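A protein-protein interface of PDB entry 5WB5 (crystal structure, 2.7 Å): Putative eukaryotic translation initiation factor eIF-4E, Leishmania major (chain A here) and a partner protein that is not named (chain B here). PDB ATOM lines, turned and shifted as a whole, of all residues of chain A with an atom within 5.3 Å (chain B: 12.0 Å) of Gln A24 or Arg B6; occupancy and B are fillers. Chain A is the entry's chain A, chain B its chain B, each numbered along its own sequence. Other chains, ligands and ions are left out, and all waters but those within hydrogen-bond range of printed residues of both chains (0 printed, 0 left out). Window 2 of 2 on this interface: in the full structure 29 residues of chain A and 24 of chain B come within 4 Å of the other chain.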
ATOM      1  N   LYS A  22     -14.035 -20.995 -18.103  1.00  0.00           N
ATOM      2  CA  LYS A  22     -13.324 -22.126 -17.529  1.00  0.00           C
ATOM      3  C   LYS A  22     -13.982 -22.599 -16.238  1.00  0.00           C
ATOM      4  O   LYS A  22     -14.533 -21.811 -15.464  1.00  0.00           O
ATOM      5  CB  LYS A  22     -11.869 -21.753 -17.259  1.00  0.00           C
ATOM      6  N   LEU A  23     -13.906 -23.908 -16.009  1.00  0.00           N
ATOM      7  CA  LEU A  23     -14.416 -24.532 -14.798  1.00  0.00           C
ATOM      8  C   LEU A  23     -13.326 -24.599 -13.735  1.00  0.00           C
ATOM      9  O   LEU A  23     -12.132 -24.496 -14.023  1.00  0.00           O
ATOM     10  CB  LEU A  23     -14.930 -25.941 -15.093  1.00  0.00           C
ATOM     11  CG  LEU A  23     -16.090 -26.067 -16.076  1.00  0.00           C
ATOM     12  CD1 LEU A  23     -16.338 -27.527 -16.395  1.00  0.00           C
ATOM     13  CD2 LEU A  23     -17.342 -25.431 -15.512  1.00  0.00           C
ATOM     14  N   GLN A  24     -13.756 -24.782 -12.486  1.00  0.00           N
ATOM     15  CA  GLN A  24     -12.793 -24.995 -11.414  1.00  0.00           C
ATOM     16  C   GLN A  24     -12.037 -26.300 -11.605  1.00  0.00           C
ATOM     17  O   GLN A  24     -10.882 -26.416 -11.183  1.00  0.00           O
ATOM     18  CB  GLN A  24     -13.503 -24.984 -10.059  1.00  0.00           C
ATOM     19  CG  GLN A  24     -12.574 -25.153  -8.865  1.00  0.00           C
ATOM     20  CD  GLN A  24     -11.519 -24.068  -8.784  1.00  0.00           C
ATOM     21  OE1 GLN A  24     -11.817 -22.882  -8.929  1.00  0.00           O
ATOM     22  NE2 GLN A  24     -10.274 -24.469  -8.558  1.00  0.00           N
ATOM     23  N   ARG A  25     -12.665 -27.286 -12.244  1.00  0.00           N
ATOM     24  CA  ARG A  25     -12.058 -28.594 -12.431  1.00  0.00           C
ATOM     25  C   ARG A  25     -12.555 -29.190 -13.739  1.00  0.00           C
ATOM     26  O   ARG A  25     -13.666 -28.897 -14.188  1.00  0.00           O
ATOM     27  CB  ARG A  25     -12.392 -29.540 -11.268  1.00  0.00           C
ATOM     28  CG  ARG A  25     -11.926 -29.051  -9.908  1.00  0.00           C
ATOM     29  CD  ARG A  25     -12.283 -30.038  -8.807  1.00  0.00           C
ATOM     30  NE  ARG A  25     -13.702 -30.008  -8.466  1.00  0.00           N
ATOM     31  CZ  ARG A  25     -14.286 -30.851  -7.618  1.00  0.00           C
ATOM     32  NH1 ARG A  25     -13.576 -31.800  -7.024  1.00  0.00           N
ATOM     33  NH2 ARG A  25     -15.582 -30.747  -7.366  1.00  0.00           N
ATOM     34  N   ALA A  26     -11.720 -30.029 -14.346  1.00  0.00           N
ATOM     35  CA  ALA A  26     -12.154 -30.816 -15.486  1.00  0.00           C
ATOM     36  C   ALA A  26     -12.991 -31.996 -15.004  1.00  0.00           C
ATOM     37  O   ALA A  26     -12.878 -32.440 -13.858  1.00  0.00           O
ATOM     38  CB  ALA A  26     -10.954 -31.310 -16.292  1.00  0.00           C
ATOM     39  N   VAL A 146     -20.562 -29.149 -11.921  1.00  0.00           N
ATOM     40  CA  VAL A 146     -19.575 -28.372 -12.669  1.00  0.00           C
ATOM     41  C   VAL A 146     -19.471 -26.957 -12.113  1.00  0.00           C
ATOM     42  O   VAL A 146     -18.381 -26.374 -12.068  1.00  0.00           O
ATOM     43  CB  VAL A 146     -19.900 -28.365 -14.175  1.00  0.00           C
ATOM     44  CG1 VAL A 146     -19.765 -29.763 -14.748  1.00  0.00           C
ATOM     45  CG2 VAL A 146     -21.285 -27.791 -14.439  1.00  0.00           C
ATOM     46  N   GLU A 148     -19.774 -26.059  -9.065  1.00  0.00           N
ATOM     47  CA  GLU A 148     -19.142 -26.088  -7.749  1.00  0.00           C
ATOM     48  C   GLU A 148     -20.046 -25.560  -6.642  1.00  0.00           C
ATOM     49  O   GLU A 148     -19.552 -25.152  -5.587  1.00  0.00           O
ATOM     50  CB  GLU A 148     -17.821 -25.306  -7.748  1.00  0.00           C
ATOM     51  CG  GLU A 148     -16.757 -25.888  -8.659  1.00  0.00           C
ATOM     52  CD  GLU A 148     -16.253 -27.233  -8.185  1.00  0.00           C
ATOM     53  OE1 GLU A 148     -16.485 -27.575  -7.004  1.00  0.00           O
ATOM     54  OE2 GLU A 148     -15.629 -27.948  -8.997  1.00  0.00           O
ATOM     55  N   TYR A 149     -21.364 -25.547  -6.849  1.00  0.00           N
ATOM     56  CA  TYR A 149     -22.298 -25.233  -5.776  1.00  0.00           C
ATOM     57  C   TYR A 149     -23.014 -26.474  -5.261  1.00  0.00           C
ATOM     58  O   TYR A 149     -24.113 -26.368  -4.704  1.00  0.00           O
ATOM     59  CB  TYR A 149     -23.307 -24.166  -6.214  1.00  0.00           C
ATOM     60  CG  TYR A 149     -24.086 -24.444  -7.480  1.00  0.00           C
ATOM     61  CD1 TYR A 149     -23.547 -24.145  -8.724  1.00  0.00           C
ATOM     62  CD2 TYR A 149     -25.380 -24.952  -7.433  1.00  0.00           C
ATOM     63  CE1 TYR A 149     -24.257 -24.370  -9.886  1.00  0.00           C
ATOM     64  CE2 TYR A 149     -26.102 -25.179  -8.596  1.00  0.00           C
ATOM     65  CZ  TYR A 149     -25.535 -24.881  -9.822  1.00  0.00           C
ATOM     66  OH  TYR A 149     -26.231 -25.105 -10.991  1.00  0.00           O
ATOM     67  N   ASP A 151     -21.159 -28.221  -3.088  1.00  0.00           N
ATOM     68  CA  ASP A 151     -20.636 -27.956  -1.749  1.00  0.00           C
ATOM     69  C   ASP A 151     -20.070 -26.541  -1.762  1.00  0.00           C
ATOM     70  O   ASP A 151     -19.019 -26.297  -2.365  1.00  0.00           O
ATOM     71  CB  ASP A 151     -19.570 -28.976  -1.347  1.00  0.00           C
ATOM     72  CG  ASP A 151     -18.417 -29.030  -2.327  1.00  0.00           C
ATOM     73  OD1 ASP A 151     -18.661 -28.859  -3.541  1.00  0.00           O
ATOM     74  OD2 ASP A 151     -17.267 -29.235  -1.882  1.00  0.00           O
ATOM     75  N   CYS A 152     -20.762 -25.611  -1.107  1.00  0.00           N
ATOM     76  CA  CYS A 152     -20.437 -24.192  -1.193  1.00  0.00           C
ATOM     77  C   CYS A 152     -19.423 -23.744  -0.146  1.00  0.00           C
ATOM     78  O   CYS A 152     -19.208 -22.535   0.004  1.00  0.00           O
ATOM     79  CB  CYS A 152     -21.711 -23.353  -1.058  1.00  0.00           C
ATOM     80  SG  CYS A 152     -22.343 -23.239   0.632  1.00  0.00           S
ATOM     81  N   VAL A 153     -18.798 -24.678   0.568  1.00  0.00           N
ATOM     82  CA  VAL A 153     -17.825 -24.368   1.618  1.00  0.00           C
ATOM     83  C   VAL A 153     -18.243 -23.144   2.429  1.00  0.00           C
ATOM     84  O   VAL A 153     -19.432 -22.911   2.656  1.00  0.00           O
ATOM     85  CB  VAL A 153     -16.404 -24.168   1.028  1.00  0.00           C
ATOM     86  CG1 VAL A 153     -15.990 -25.386   0.210  1.00  0.00           C
ATOM     87  CG2 VAL A 153     -16.312 -22.892   0.188  1.00  0.00           C
ATOM     88  N   VAL B   5     -13.498 -19.403  -2.040  1.00  0.00           N
ATOM     89  CA  VAL B   5     -12.710 -18.652  -3.010  1.00  0.00           C
ATOM     90  C   VAL B   5     -12.237 -19.579  -4.129  1.00  0.00           C
ATOM     91  O   VAL B   5     -11.098 -20.050  -4.121  1.00  0.00           O
ATOM     92  CB  VAL B   5     -11.515 -17.949  -2.332  1.00  0.00           C
ATOM     93  CG1 VAL B   5     -10.709 -17.139  -3.345  1.00  0.00           C
ATOM     94  CG2 VAL B   5     -11.999 -17.050  -1.200  1.00  0.00           C
ATOM     95  N   ARG B   6     -13.121 -19.837  -5.089  1.00  0.00           N
ATOM     96  CA  ARG B   6     -12.799 -20.689  -6.225  1.00  0.00           C
ATOM     97  C   ARG B   6     -13.758 -20.362  -7.362  1.00  0.00           C
ATOM     98  O   ARG B   6     -14.742 -19.642  -7.184  1.00  0.00           O
ATOM     99  CB  ARG B   6     -12.872 -22.174  -5.850  1.00  0.00           C
ATOM    100  CG  ARG B   6     -14.234 -22.625  -5.339  1.00  0.00           C
ATOM    101  CD  ARG B   6     -14.237 -24.112  -5.009  1.00  0.00           C
ATOM    102  NE  ARG B   6     -15.547 -24.572  -4.554  1.00  0.00           N
ATOM    103  CZ  ARG B   6     -15.852 -25.841  -4.296  1.00  0.00           C
ATOM    104  NH1 ARG B   6     -14.942 -26.794  -4.446  1.00  0.00           N
ATOM    105  NH2 ARG B   6     -17.073 -26.160  -3.888  1.00  0.00           N
ATOM    106  N   THR B   7     -13.456 -20.909  -8.538  1.00  0.00           N
ATOM    107  CA  THR B   7     -14.261 -20.656  -9.731  1.00  0.00           C
ATOM    108  C   THR B   7     -15.648 -21.259  -9.539  1.00  0.00           C
ATOM    109  O   THR B   7     -15.814 -22.482  -9.601  1.00  0.00           O
ATOM    110  CB  THR B   7     -13.578 -21.242 -10.963  1.00  0.00           C
ATOM    111  OG1 THR B   7     -12.264 -20.683 -11.096  1.00  0.00           O
ATOM    112  CG2 THR B   7     -14.378 -20.941 -12.222  1.00  0.00           C
ATOM    113  N   MET B   8     -16.643 -20.407  -9.307  1.00  0.00           N
ATOM    114  CA  MET B   8     -18.012 -20.842  -9.080  1.00  0.00           C
ATOM    115  C   MET B   8     -18.948 -20.216 -10.104  1.00  0.00           C
ATOM    116  O   MET B   8     -18.721 -19.103 -10.585  1.00  0.00           O
ATOM    117  CB  MET B   8     -18.489 -20.474  -7.670  1.00  0.00           C
ATOM    118  CG  MET B   8     -17.874 -21.304  -6.553  1.00  0.00           C
ATOM    119  SD  MET B   8     -18.718 -21.037  -4.981  1.00  0.00           S
ATOM    120  CE  MET B   8     -17.854 -22.177  -3.908  1.00  0.00           C
ATOM    121  N   TYR B   9     -20.006 -20.954 -10.429  1.00  0.00           N
ATOM    122  CA  TYR B   9     -21.078 -20.473 -11.284  1.00  0.00           C
ATOM    123  C   TYR B   9     -22.411 -20.807 -10.634  1.00  0.00           C
ATOM    124  O   TYR B   9     -22.526 -21.779  -9.885  1.00  0.00           O
ATOM    125  CB  TYR B   9     -21.030 -21.104 -12.687  1.00  0.00           C
ATOM    126  CG  TYR B   9     -19.797 -20.757 -13.489  1.00  0.00           C
ATOM    127  CD1 TYR B   9     -18.662 -21.549 -13.424  1.00  0.00           C
ATOM    128  CD2 TYR B   9     -19.772 -19.642 -14.316  1.00  0.00           C
ATOM    129  CE1 TYR B   9     -17.531 -21.241 -14.155  1.00  0.00           C
ATOM    130  CE2 TYR B   9     -18.646 -19.323 -15.051  1.00  0.00           C
ATOM    131  CZ  TYR B   9     -17.526 -20.129 -14.967  1.00  0.00           C
ATOM    132  OH  TYR B   9     -16.393 -19.832 -15.691  1.00  0.00           O
ATOM    133  N   THR B  10     -23.414 -19.990 -10.921  1.00  0.00           N
ATOM    134  CA  THR B  10     -24.780 -20.265 -10.507  1.00  0.00           C
ATOM    135  C   THR B  10     -25.520 -20.965 -11.640  1.00  0.00           C
ATOM    136  O   THR B  10     -25.099 -20.938 -12.799  1.00  0.00           O
ATOM    137  CB  THR B  10     -25.519 -18.975 -10.121  1.00  0.00           C
ATOM    138  OG1 THR B  10     -25.687 -18.146 -11.280  1.00  0.00           O
ATOM    139  CG2 THR B  10     -24.749 -18.201  -9.045  1.00  0.00           C
ATOM    140  N   GLU B  13     -26.439 -18.509 -14.278  1.00  0.00           N
ATOM    141  CA  GLU B  13     -25.257 -18.130 -15.046  1.00  0.00           C
ATOM    142  C   GLU B  13     -24.880 -19.217 -16.048  1.00  0.00           C
ATOM    143  O   GLU B  13     -24.540 -18.923 -17.202  1.00  0.00           O
ATOM    144  CB  GLU B  13     -24.099 -17.843 -14.089  1.00  0.00           C
ATOM    145  CG  GLU B  13     -22.893 -17.183 -14.734  1.00  0.00           C
ATOM    146  CD  GLU B  13     -21.948 -16.568 -13.712  1.00  0.00           C
ATOM    147  OE1 GLU B  13     -22.118 -16.828 -12.503  1.00  0.00           O
ATOM    148  OE2 GLU B  13     -21.037 -15.817 -14.118  1.00  0.00           O
ATOM    149  N   LEU B  14     -24.937 -20.484 -15.628  1.00  0.00           N
ATOM    150  CA  LEU B  14     -24.658 -21.582 -16.547  1.00  0.00           C
ATOM    151  C   LEU B  14     -25.669 -21.610 -17.684  1.00  0.00           C
ATOM    152  O   LEU B  14     -25.305 -21.825 -18.846  1.00  0.00           O
ATOM    153  CB  LEU B  14     -24.671 -22.914 -15.792  1.00  0.00           C
ATOM    154  CG  LEU B  14     -23.657 -23.072 -14.654  1.00  0.00           C
ATOM    155  CD1 LEU B  14     -24.007 -24.277 -13.792  1.00  0.00           C
ATOM    156  CD2 LEU B  14     -22.247 -23.197 -15.200  1.00  0.00           C
ATOM    157  N   ILE B  17     -24.731 -18.978 -20.135  1.00  0.00           N
ATOM    158  CA  ILE B  17     -23.572 -19.355 -20.941  1.00  0.00           C
ATOM    159  C   ILE B  17     -23.915 -20.457 -21.939  1.00  0.00           C
ATOM    160  O   ILE B  17     -23.222 -20.613 -22.954  1.00  0.00           O
ATOM    161  CB  ILE B  17     -22.403 -19.786 -20.034  1.00  0.00           C
ATOM    162  CG1 ILE B  17     -22.012 -18.644 -19.096  1.00  0.00           C
ATOM    163  CG2 ILE B  17     -21.193 -20.193 -20.870  1.00  0.00           C
ATOM    164  CD1 ILE B  17     -21.073 -19.056 -17.981  1.00  0.00           C
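O of Lys A22 touches CG2 of Thr B7, at 3.4 Å.
OE1 of Gln A24 touches CB of Arg B6 (3.3 Å).
Glu A148 touches Thr B7.
Glu A148 touches Met B8 (O to CE, 3.8 Å).
O of Tyr B9 touches CD1 of Tyr A149, at 2.8 Å.
CD1 of Leu B14 touches OH of Tyr A149, 3.7 Å away.
The guanidinium group (NE) of Arg A25 is in salt-bridge range of the side-chain carboxylate (OE2) of Glu A148.
Gln A24 touches just these residues of chain B: Arg B6 (3.3 Å) and Thr B7 (2.6 Å).
Arg B6 touches just these residues of chain A: Gln A24, Glu A148 and Asp A151.
Lys A22 touches just these residues of chain B: Thr B7 and Tyr B9.
No residue of chain B comes within 4 Å of Ala A26.
Of chain B, only Arg B6 (3.1 Å), Thr B7 (3.7 Å) and Met B8 (3.8 Å) come within 4 Å of Glu A148.
Asp A151 touches just one residue of chain B: Arg B6.
No residue of chain B comes within 4 Å of Cys A152.
Val A153 touches none of the printed residues of chain B.
Printed residues of chain B within 4 Å of Tyr A149: Tyr B9 and Leu B14.
Printed residues of chain A within 4 Å of Thr B7: Lys A22 (3.4 Å), Gln A24 (2.6 Å) and Glu A148 (3.7 Å).
Of the printed residues of chain A, Tyr B9 touches Lys A22 (2.7 Å) and Tyr A149 (2.8 Å).
Printed residues of chain A within 4 Å of Leu B14: Tyr A149.
Printed residues of chain A within 4 Å of Met B8: Glu A148.
Ile B17 touches none of the printed residues of chain A.
Val B5 touches none of the printed residues of chain A.
The nearest printed residue of chain B that does not touch Gln A24 is Met B8 (5.4 Å).
The nearest residue of chain A that does not touch Arg B6 is Val A153 (4.3 Å).
Of the 9 printed residues of chain B, 5 touch a printed residue of chain A.
Hydrophobic or aromatic side chains of chain B within 4 Å of the printed part of chain A: Met B8, Tyr B9 and Leu B14.
Of the 11 printed residues of chain A, 5 touch a printed residue of chain B.
Among the printed residues, Asp or Glu carboxylates within 4 Å of a Lys or Arg side-chain nitrogen of the other chain: Glu A148 with Arg B6 (3.1 Å) and Asp A151 with Arg B6 (3.2 Å).
OE1 of Glu A148 is in salt-bridge range of NH1 of Arg B6, at 3.1 Å.
OE1 of Gln A24 sits at hydrogen-bond distance from N of Thr B7 (2.6 Å).
OD1 of Asp A151 lies within salt-bridge range of NH2 of Arg B6, 3.2 Å away.
O of Lys A22 sits at hydrogen-bond distance from OH of Tyr B9 (2.7 Å).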
